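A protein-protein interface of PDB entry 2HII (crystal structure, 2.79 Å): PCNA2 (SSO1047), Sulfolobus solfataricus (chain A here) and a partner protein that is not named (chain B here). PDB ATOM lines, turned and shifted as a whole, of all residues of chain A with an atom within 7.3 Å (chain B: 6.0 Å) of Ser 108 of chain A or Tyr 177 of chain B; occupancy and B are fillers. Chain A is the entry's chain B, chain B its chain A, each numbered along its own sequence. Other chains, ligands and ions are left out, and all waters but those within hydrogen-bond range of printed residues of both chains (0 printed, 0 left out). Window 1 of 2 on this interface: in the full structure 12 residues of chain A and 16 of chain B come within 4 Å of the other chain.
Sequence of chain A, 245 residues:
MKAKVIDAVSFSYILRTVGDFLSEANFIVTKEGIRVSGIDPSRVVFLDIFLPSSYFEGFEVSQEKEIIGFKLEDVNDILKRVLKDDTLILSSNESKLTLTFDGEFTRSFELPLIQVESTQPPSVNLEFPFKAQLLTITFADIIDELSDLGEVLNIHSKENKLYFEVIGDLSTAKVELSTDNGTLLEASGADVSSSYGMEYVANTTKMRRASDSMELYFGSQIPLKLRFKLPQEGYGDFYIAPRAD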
ATOM      1  N   ILE A  78     -22.477 -14.423 -25.329  1.00  0.00           N
ATOM      2  CA  ILE A  78     -21.116 -14.101 -24.930  1.00  0.00           C
ATOM      3  C   ILE A  78     -20.737 -14.869 -23.663  1.00  0.00           C
ATOM      4  O   ILE A  78     -19.615 -15.341 -23.541  1.00  0.00           O
ATOM      5  CB  ILE A  78     -20.837 -12.558 -24.836  1.00  0.00           C
ATOM      6  CG1 ILE A  78     -20.841 -12.053 -23.401  1.00  0.00           C
ATOM      7  CG2 ILE A  78     -21.771 -11.746 -25.732  1.00  0.00           C
ATOM      8  CD1 ILE A  78     -19.469 -11.963 -22.834  1.00  0.00           C
ATOM      9  N   ILE A  89     -15.349  -9.370 -15.089  1.00  0.00           N
ATOM     10  CA  ILE A  89     -15.477  -7.953 -14.774  1.00  0.00           C
ATOM     11  C   ILE A  89     -16.501  -7.361 -15.735  1.00  0.00           C
ATOM     12  O   ILE A  89     -16.215  -7.179 -16.921  1.00  0.00           O
ATOM     13  CB  ILE A  89     -14.126  -7.210 -14.916  1.00  0.00           C
ATOM     14  CG1 ILE A  89     -13.225  -7.520 -13.721  1.00  0.00           C
ATOM     15  CG2 ILE A  89     -14.331  -5.702 -15.069  1.00  0.00           C
ATOM     16  CD1 ILE A  89     -11.874  -6.813 -13.733  1.00  0.00           C
ATOM     17  N   THR A  98     -19.870  -3.878 -21.375  1.00  0.00           N
ATOM     18  CA  THR A  98     -18.750  -4.710 -21.747  1.00  0.00           C
ATOM     19  C   THR A  98     -18.518  -5.788 -20.717  1.00  0.00           C
ATOM     20  O   THR A  98     -18.539  -5.524 -19.514  1.00  0.00           O
ATOM     21  CB  THR A  98     -17.429  -3.909 -21.993  1.00  0.00           C
ATOM     22  OG1 THR A  98     -16.343  -4.561 -21.322  1.00  0.00           O
ATOM     23  CG2 THR A  98     -17.515  -2.485 -21.492  1.00  0.00           C
ATOM     24  N   LEU A  99     -18.292  -7.003 -21.207  1.00  0.00           N
ATOM     25  CA  LEU A  99     -17.981  -8.152 -20.362  1.00  0.00           C
ATOM     26  C   LEU A  99     -16.541  -8.601 -20.589  1.00  0.00           C
ATOM     27  O   LEU A  99     -16.137  -8.856 -21.720  1.00  0.00           O
ATOM     28  CB  LEU A  99     -18.955  -9.297 -20.630  1.00  0.00           C
ATOM     29  CG  LEU A  99     -20.450  -8.962 -20.608  1.00  0.00           C
ATOM     30  CD1 LEU A  99     -20.951  -8.530 -21.979  1.00  0.00           C
ATOM     31  CD2 LEU A  99     -21.231 -10.158 -20.139  1.00  0.00           C
ATOM     32  N   THR A 100     -15.771  -8.685 -19.506  1.00  0.00           N
ATOM     33  CA  THR A 100     -14.359  -9.061 -19.580  1.00  0.00           C
ATOM     34  C   THR A 100     -14.046 -10.282 -18.726  1.00  0.00           C
ATOM     35  O   THR A 100     -14.274 -10.277 -17.512  1.00  0.00           O
ATOM     36  CB  THR A 100     -13.437  -7.906 -19.154  1.00  0.00           C
ATOM     37  OG1 THR A 100     -13.819  -6.703 -19.838  1.00  0.00           O
ATOM     38  CG2 THR A 100     -11.985  -8.232 -19.486  1.00  0.00           C
ATOM     39  N   PHE A 101     -13.533 -11.323 -19.380  1.00  0.00           N
ATOM     40  CA  PHE A 101     -13.132 -12.557 -18.722  1.00  0.00           C
ATOM     41  C   PHE A 101     -11.653 -12.541 -18.397  1.00  0.00           C
ATOM     42  O   PHE A 101     -10.846 -12.055 -19.181  1.00  0.00           O
ATOM     43  CB  PHE A 101     -13.441 -13.751 -19.606  1.00  0.00           C
ATOM     44  CG  PHE A 101     -14.884 -13.886 -19.949  1.00  0.00           C
ATOM     45  CD1 PHE A 101     -15.324 -13.657 -21.242  1.00  0.00           C
ATOM     46  CD2 PHE A 101     -15.811 -14.243 -18.979  1.00  0.00           C
ATOM     47  CE1 PHE A 101     -16.666 -13.791 -21.579  1.00  0.00           C
ATOM     48  CE2 PHE A 101     -17.163 -14.376 -19.300  1.00  0.00           C
ATOM     49  CZ  PHE A 101     -17.590 -14.149 -20.607  1.00  0.00           C
ATOM     50  N   PHE A 105      -6.041 -16.041 -20.053  1.00  0.00           N
ATOM     51  CA  PHE A 105      -5.737 -14.751 -20.682  1.00  0.00           C
ATOM     52  C   PHE A 105      -6.974 -13.841 -20.645  1.00  0.00           C
ATOM     53  O   PHE A 105      -8.094 -14.317 -20.476  1.00  0.00           O
ATOM     54  CB  PHE A 105      -5.200 -14.932 -22.115  1.00  0.00           C
ATOM     55  CG  PHE A 105      -6.198 -15.509 -23.083  1.00  0.00           C
ATOM     56  CD1 PHE A 105      -6.673 -14.743 -24.138  1.00  0.00           C
ATOM     57  CD2 PHE A 105      -6.668 -16.806 -22.935  1.00  0.00           C
ATOM     58  CE1 PHE A 105      -7.593 -15.260 -25.026  1.00  0.00           C
ATOM     59  CE2 PHE A 105      -7.593 -17.321 -23.812  1.00  0.00           C
ATOM     60  CZ  PHE A 105      -8.054 -16.549 -24.861  1.00  0.00           C
ATOM     61  N   THR A 106      -6.761 -12.539 -20.793  1.00  0.00           N
ATOM     62  CA  THR A 106      -7.837 -11.563 -20.713  1.00  0.00           C
ATOM     63  C   THR A 106      -8.614 -11.479 -22.021  1.00  0.00           C
ATOM     64  O   THR A 106      -8.030 -11.446 -23.100  1.00  0.00           O
ATOM     65  CB  THR A 106      -7.300 -10.180 -20.338  1.00  0.00           C
ATOM     66  OG1 THR A 106      -6.163 -10.333 -19.483  1.00  0.00           O
ATOM     67  CG2 THR A 106      -8.367  -9.366 -19.613  1.00  0.00           C
ATOM     68  N   ARG A 107      -9.936 -11.444 -21.906  1.00  0.00           N
ATOM     69  CA  ARG A 107     -10.839 -11.459 -23.045  1.00  0.00           C
ATOM     70  C   ARG A 107     -12.003 -10.545 -22.760  1.00  0.00           C
ATOM     71  O   ARG A 107     -12.632 -10.671 -21.714  1.00  0.00           O
ATOM     72  CB  ARG A 107     -11.409 -12.860 -23.232  1.00  0.00           C
ATOM     73  CG  ARG A 107     -10.431 -13.876 -23.740  1.00  0.00           C
ATOM     74  CD  ARG A 107     -11.116 -15.202 -23.939  1.00  0.00           C
ATOM     75  NE  ARG A 107     -11.647 -15.714 -22.683  1.00  0.00           N
ATOM     76  CZ  ARG A 107     -12.779 -16.390 -22.585  1.00  0.00           C
ATOM     77  NH1 ARG A 107     -13.511 -16.621 -23.662  1.00  0.00           N
ATOM     78  NH2 ARG A 107     -13.190 -16.824 -21.404  1.00  0.00           N
ATOM     79  N   SER A 108     -12.326  -9.643 -23.676  1.00  0.00           N
ATOM     80  CA  SER A 108     -13.497  -8.809 -23.456  1.00  0.00           C
ATOM     81  C   SER A 108     -14.449  -8.728 -24.643  1.00  0.00           C
ATOM     82  O   SER A 108     -14.038  -8.700 -25.802  1.00  0.00           O
ATOM     83  CB  SER A 108     -13.113  -7.410 -22.952  1.00  0.00           C
ATOM     84  OG  SER A 108     -12.439  -6.666 -23.952  1.00  0.00           O
ATOM     85  N   PHE A 109     -15.737  -8.699 -24.317  1.00  0.00           N
ATOM     86  CA  PHE A 109     -16.804  -8.576 -25.300  1.00  0.00           C
ATOM     87  C   PHE A 109     -17.642  -7.329 -25.042  1.00  0.00           C
ATOM     88  O   PHE A 109     -18.037  -7.043 -23.911  1.00  0.00           O
ATOM     89  CB  PHE A 109     -17.703  -9.814 -25.282  1.00  0.00           C
ATOM     90  CG  PHE A 109     -16.981 -11.098 -25.613  1.00  0.00           C
ATOM     91  CD1 PHE A 109     -16.259 -11.780 -24.642  1.00  0.00           C
ATOM     92  CD2 PHE A 109     -17.031 -11.622 -26.893  1.00  0.00           C
ATOM     93  CE1 PHE A 109     -15.606 -12.937 -24.934  1.00  0.00           C
ATOM     94  CE2 PHE A 109     -16.376 -12.792 -27.192  1.00  0.00           C
ATOM     95  CZ  PHE A 109     -15.659 -13.448 -26.207  1.00  0.00           C
ATOM     96  N   GLU A 110     -17.911  -6.594 -26.110  1.00  0.00           N
ATOM     97  CA  GLU A 110     -18.664  -5.363 -26.044  1.00  0.00           C
ATOM     98  C   GLU A 110     -20.063  -5.646 -26.542  1.00  0.00           C
ATOM     99  O   GLU A 110     -20.249  -6.418 -27.477  1.00  0.00           O
ATOM    100  CB  GLU A 110     -17.996  -4.318 -26.933  1.00  0.00           C
ATOM    101  CG  GLU A 110     -17.752  -2.992 -26.252  1.00  0.00           C
ATOM    102  CD  GLU A 110     -16.389  -2.405 -26.590  1.00  0.00           C
ATOM    103  OE1 GLU A 110     -15.681  -1.994 -25.637  1.00  0.00           O
ATOM    104  OE2 GLU A 110     -16.026  -2.362 -27.794  1.00  0.00           O
ATOM    105  N   VAL B 145     -10.596 -21.474 -28.285  1.00  0.00           N
ATOM    106  CA  VAL B 145     -11.328 -20.450 -27.558  1.00  0.00           C
ATOM    107  C   VAL B 145     -11.382 -19.206 -28.424  1.00  0.00           C
ATOM    108  O   VAL B 145     -12.426 -18.586 -28.578  1.00  0.00           O
ATOM    109  CB  VAL B 145     -10.657 -20.096 -26.208  1.00  0.00           C
ATOM    110  CG1 VAL B 145     -11.549 -19.185 -25.383  1.00  0.00           C
ATOM    111  CG2 VAL B 145     -10.322 -21.345 -25.419  1.00  0.00           C
ATOM    112  N   ILE B 146     -10.245 -18.866 -29.011  1.00  0.00           N
ATOM    113  CA  ILE B 146     -10.128 -17.643 -29.777  1.00  0.00           C
ATOM    114  C   ILE B 146     -11.042 -17.720 -30.987  1.00  0.00           C
ATOM    115  O   ILE B 146     -11.850 -16.824 -31.218  1.00  0.00           O
ATOM    116  CB  ILE B 146      -8.665 -17.350 -30.163  1.00  0.00           C
ATOM    117  CG1 ILE B 146      -7.829 -17.086 -28.897  1.00  0.00           C
ATOM    118  CG2 ILE B 146      -8.596 -16.147 -31.102  1.00  0.00           C
ATOM    119  CD1 ILE B 146      -6.338 -16.942 -29.132  1.00  0.00           C
ATOM    120  N   ASP B 149     -14.846 -17.334 -30.033  1.00  0.00           N
ATOM    121  CA  ASP B 149     -15.384 -16.040 -29.678  1.00  0.00           C
ATOM    122  C   ASP B 149     -15.079 -14.970 -30.706  1.00  0.00           C
ATOM    123  O   ASP B 149     -15.749 -13.935 -30.743  1.00  0.00           O
ATOM    124  CB  ASP B 149     -15.173 -15.612 -28.200  1.00  0.00           C
ATOM    125  CG  ASP B 149     -13.778 -15.861 -27.679  1.00  0.00           C
ATOM    126  OD1 ASP B 149     -12.820 -15.350 -28.287  1.00  0.00           O
ATOM    127  OD2 ASP B 149     -13.653 -16.528 -26.628  1.00  0.00           O
ATOM    128  N   VAL B 150     -14.114 -15.238 -31.574  1.00  0.00           N
ATOM    129  CA  VAL B 150     -13.943 -14.396 -32.755  1.00  0.00           C
ATOM    130  C   VAL B 150     -15.135 -14.563 -33.702  1.00  0.00           C
ATOM    131  O   VAL B 150     -15.684 -13.572 -34.160  1.00  0.00           O
ATOM    132  CB  VAL B 150     -12.588 -14.639 -33.454  1.00  0.00           C
ATOM    133  CG1 VAL B 150     -12.615 -14.206 -34.928  1.00  0.00           C
ATOM    134  CG2 VAL B 150     -11.480 -13.923 -32.695  1.00  0.00           C
ATOM    135  N   VAL B 153     -18.590 -12.713 -32.956  1.00  0.00           N
ATOM    136  CA  VAL B 153     -18.709 -11.257 -33.120  1.00  0.00           C
ATOM    137  C   VAL B 153     -18.572 -10.775 -34.576  1.00  0.00           C
ATOM    138  O   VAL B 153     -19.056  -9.683 -34.924  1.00  0.00           O
ATOM    139  CB  VAL B 153     -17.725 -10.464 -32.188  1.00  0.00           C
ATOM    140  CG1 VAL B 153     -17.845 -10.917 -30.740  1.00  0.00           C
ATOM    141  CG2 VAL B 153     -16.293 -10.589 -32.664  1.00  0.00           C
ATOM    142  N   ILE B 168      -5.702  -9.511 -30.366  1.00  0.00           N
ATOM    143  CA  ILE B 168      -6.655 -10.107 -31.284  1.00  0.00           C
ATOM    144  C   ILE B 168      -7.951  -9.366 -31.086  1.00  0.00           C
ATOM    145  O   ILE B 168      -8.516  -9.355 -29.998  1.00  0.00           O
ATOM    146  CB  ILE B 168      -6.780 -11.644 -31.053  1.00  0.00           C
ATOM    147  CG1 ILE B 168      -5.621 -12.362 -31.751  1.00  0.00           C
ATOM    148  CG2 ILE B 168      -8.083 -12.197 -31.591  1.00  0.00           C
ATOM    149  CD1 ILE B 168      -5.085 -13.579 -31.021  1.00  0.00           C
ATOM    150  N   GLU B 169      -8.392  -8.690 -32.130  1.00  0.00           N
ATOM    151  CA  GLU B 169      -9.681  -8.044 -32.089  1.00  0.00           C
ATOM    152  C   GLU B 169     -10.494  -8.497 -33.268  1.00  0.00           C
ATOM    153  O   GLU B 169      -9.949  -8.905 -34.287  1.00  0.00           O
ATOM    154  CB  GLU B 169      -9.565  -6.521 -32.035  1.00  0.00           C
ATOM    155  CG  GLU B 169      -8.597  -5.910 -33.021  1.00  0.00           C
ATOM    156  CD  GLU B 169      -8.826  -4.423 -33.199  1.00  0.00           C
ATOM    157  OE1 GLU B 169      -9.187  -3.753 -32.200  1.00  0.00           O
ATOM    158  OE2 GLU B 169      -8.650  -3.928 -34.337  1.00  0.00           O
ATOM    159  N   ALA B 170     -11.805  -8.462 -33.101  1.00  0.00           N
ATOM    160  CA  ALA B 170     -12.721  -8.792 -34.168  1.00  0.00           C
ATOM    161  C   ALA B 170     -14.011  -8.067 -33.893  1.00  0.00           C
ATOM    162  O   ALA B 170     -14.218  -7.592 -32.781  1.00  0.00           O
ATOM    163  CB  ALA B 170     -12.946 -10.285 -34.235  1.00  0.00           C
ATOM    164  N   GLY B 171     -14.859  -7.969 -34.918  1.00  0.00           N
ATOM    165  CA  GLY B 171     -16.174  -7.316 -34.817  1.00  0.00           C
ATOM    166  C   GLY B 171     -16.230  -5.916 -35.411  1.00  0.00           C
ATOM    167  O   GLY B 171     -15.217  -5.378 -35.853  1.00  0.00           O
ATOM    168  N   LYS B 175     -20.501  -4.364 -31.523  1.00  0.00           N
ATOM    169  CA  LYS B 175     -20.074  -5.453 -30.644  1.00  0.00           C
ATOM    170  C   LYS B 175     -18.651  -5.904 -30.933  1.00  0.00           C
ATOM    171  O   LYS B 175     -18.454  -6.851 -31.688  1.00  0.00           O
ATOM    172  CB  LYS B 175     -21.002  -6.670 -30.787  1.00  0.00           C
ATOM    173  CG  LYS B 175     -22.421  -6.361 -31.256  1.00  0.00           C
ATOM    174  CD  LYS B 175     -23.189  -7.637 -31.603  1.00  0.00           C
ATOM    175  CE  LYS B 175     -24.610  -7.314 -32.035  1.00  0.00           C
ATOM    176  NZ  LYS B 175     -25.384  -8.537 -32.324  1.00  0.00           N
ATOM    177  N   ARG B 176     -17.665  -5.254 -30.317  1.00  0.00           N
ATOM    178  CA  ARG B 176     -16.263  -5.638 -30.509  1.00  0.00           C
ATOM    179  C   ARG B 176     -15.758  -6.760 -29.582  1.00  0.00           C
ATOM    180  O   ARG B 176     -16.210  -6.899 -28.449  1.00  0.00           O
ATOM    181  CB  ARG B 176     -15.351  -4.416 -30.415  1.00  0.00           C
ATOM    182  CG  ARG B 176     -15.456  -3.501 -31.621  1.00  0.00           C
ATOM    183  CD  ARG B 176     -14.109  -2.884 -31.992  1.00  0.00           C
ATOM    184  NE  ARG B 176     -14.170  -2.201 -33.286  1.00  0.00           N
ATOM    185  CZ  ARG B 176     -14.522  -0.929 -33.444  1.00  0.00           C
ATOM    186  NH1 ARG B 176     -14.847  -0.183 -32.391  1.00  0.00           N
ATOM    187  NH2 ARG B 176     -14.551  -0.401 -34.657  1.00  0.00           N
ATOM    188  N   TYR B 177     -14.820  -7.559 -30.083  1.00  0.00           N
ATOM    189  CA  TYR B 177     -14.063  -8.488 -29.253  1.00  0.00           C
ATOM    190  C   TYR B 177     -12.592  -8.100 -29.300  1.00  0.00           C
ATOM    191  O   TYR B 177     -12.079  -7.731 -30.358  1.00  0.00           O
ATOM    192  CB  TYR B 177     -14.243  -9.935 -29.724  1.00  0.00           C
ATOM    193  CG  TYR B 177     -13.253 -10.916 -29.128  1.00  0.00           C
ATOM    194  CD1 TYR B 177     -13.326 -11.266 -27.783  1.00  0.00           C
ATOM    195  CD2 TYR B 177     -12.243 -11.492 -29.910  1.00  0.00           C
ATOM    196  CE1 TYR B 177     -12.430 -12.163 -27.223  1.00  0.00           C
ATOM    197  CE2 TYR B 177     -11.332 -12.395 -29.358  1.00  0.00           C
ATOM    198  CZ  TYR B 177     -11.434 -12.721 -28.005  1.00  0.00           C
ATOM    199  OH  TYR B 177     -10.558 -13.610 -27.417  1.00  0.00           O
ATOM    200  N   VAL B 178     -11.930  -8.178 -28.145  1.00  0.00           N
ATOM    201  CA  VAL B 178     -10.506  -7.885 -28.017  1.00  0.00           C
ATOM    202  C   VAL B 178      -9.861  -8.842 -27.023  1.00  0.00           C
ATOM    203  O   VAL B 178     -10.286  -8.942 -25.867  1.00  0.00           O
ATOM    204  CB  VAL B 178     -10.247  -6.435 -27.530  1.00  0.00           C
ATOM    205  CG1 VAL B 178      -8.778  -6.231 -27.204  1.00  0.00           C
ATOM    206  CG2 VAL B 178     -10.699  -5.407 -28.566  1.00  0.00           C
ATOM    207  N   ALA B 179      -8.823  -9.532 -27.481  1.00  0.00           N
ATOM    208  CA  ALA B 179      -8.048 -10.415 -26.631  1.00  0.00           C
ATOM    209  C   ALA B 179      -6.585 -10.014 -26.628  1.00  0.00           C
ATOM    210  O   ALA B 179      -6.030  -9.634 -27.662  1.00  0.00           O
ATOM    211  CB  ALA B 179      -8.177 -11.827 -27.109  1.00  0.00           C
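NH1 of Arg 107 of chain A is in salt-bridge range of OD2 of Asp 149 of chain B, at 3.0 Å. The backbone carbonyl oxygen of Arg 176 of chain B sits at hydrogen-bond distance from the backbone NH of Glu 110 of chain A (2.9 Å). The backbone carbonyl oxygen (O) of Val 178 of chain B is in hydrogen-bond range of the backbone NH (N) of Ser 108 of chain A (3.1 Å).
OH of Tyr 177 of chain B sits at hydrogen-bond distance from OD1 of Asp 149 of chain B (3.0 Å). The backbone carbonyl oxygen of Ile 168 of chain B lies within hydrogen-bond range of the backbone NH of Ala 179 of chain B (2.5 Å). The backbone carbonyl oxygen (O) of Ala 170 of chain B is in hydrogen-bond range of the backbone NH (N) of Tyr 177 of chain B. N of Phe 109 of chain A sits at hydrogen-bond distance from O of Leu 99 of chain A (2.6 Å). The backbone NH of Phe 101 of chain A is in hydrogen-bond range of the backbone carbonyl oxygen of Arg 107 of chain A (2.6 Å).
Thr 106 of chain A touches Ala 179 of chain B. Arg 107 of chain A touches Val 145 of chain B. Arg 107 of chain A touches Tyr 177 of chain B. Arg 107 of chain A touches Val 178 of chain B (CA to O, 3.8 Å). Ser 108 of chain A touches Tyr 177 of chain B. CB of Asp 149 of chain B touches CZ of Phe 109 of chain A, at 3.0 Å. Phe 109 of chain A touches Val 153 of chain B. CA of Phe 109 of chain A touches O of Arg 176 of chain B, at 3.6 Å. Phe 109 of chain A touches Tyr 177 of chain B (CE2 to CD1, 3.5 Å). CA of Lys 175 of chain B touches O of Glu 110 of chain A, at 3.3 Å.
Phe 101 of chain A touches none of the printed residues of chain B. Phe 105 of chain A touches none of the printed residues of chain B. Of the printed residues of chain B, Phe 109 of chain A touches Asp 149 (3.0 Å), Val 153 (3.99 Å), Arg 176 (3.6 Å) and Tyr 177 (3.5 Å). Printed residues of chain B within 4 Å of Glu 110 of chain A: Lys 175 (3.3 Å) and Arg 176 (2.9 Å). Of the printed residues of chain A, Val 145 of chain B touches Arg 107. Printed residues of chain A within 4 Å of Val 153 of chain B: Phe 109 (3.99 Å). Of the printed residues of chain A, Lys 175 of chain B touches Glu 110 (3.3 Å). Of chain A, only Arg 107, Ser 108 and Phe 109 come within 4 Å of Tyr 177 of chain B. The nearest residue of chain B that does not touch Ser 108 of chain A is Ala 179 of chain B (5.2 Å). The nearest residue of chain A that does not touch Tyr 177 of chain B is Phe 105 of chain A (4.2 Å). The nearest printed residue of chain A that does not touch Val 153 of chain B is Glu 110 of chain A (6.1 Å).
Of the 14 printed residues of chain B, 8 touch a printed residue of chain A.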
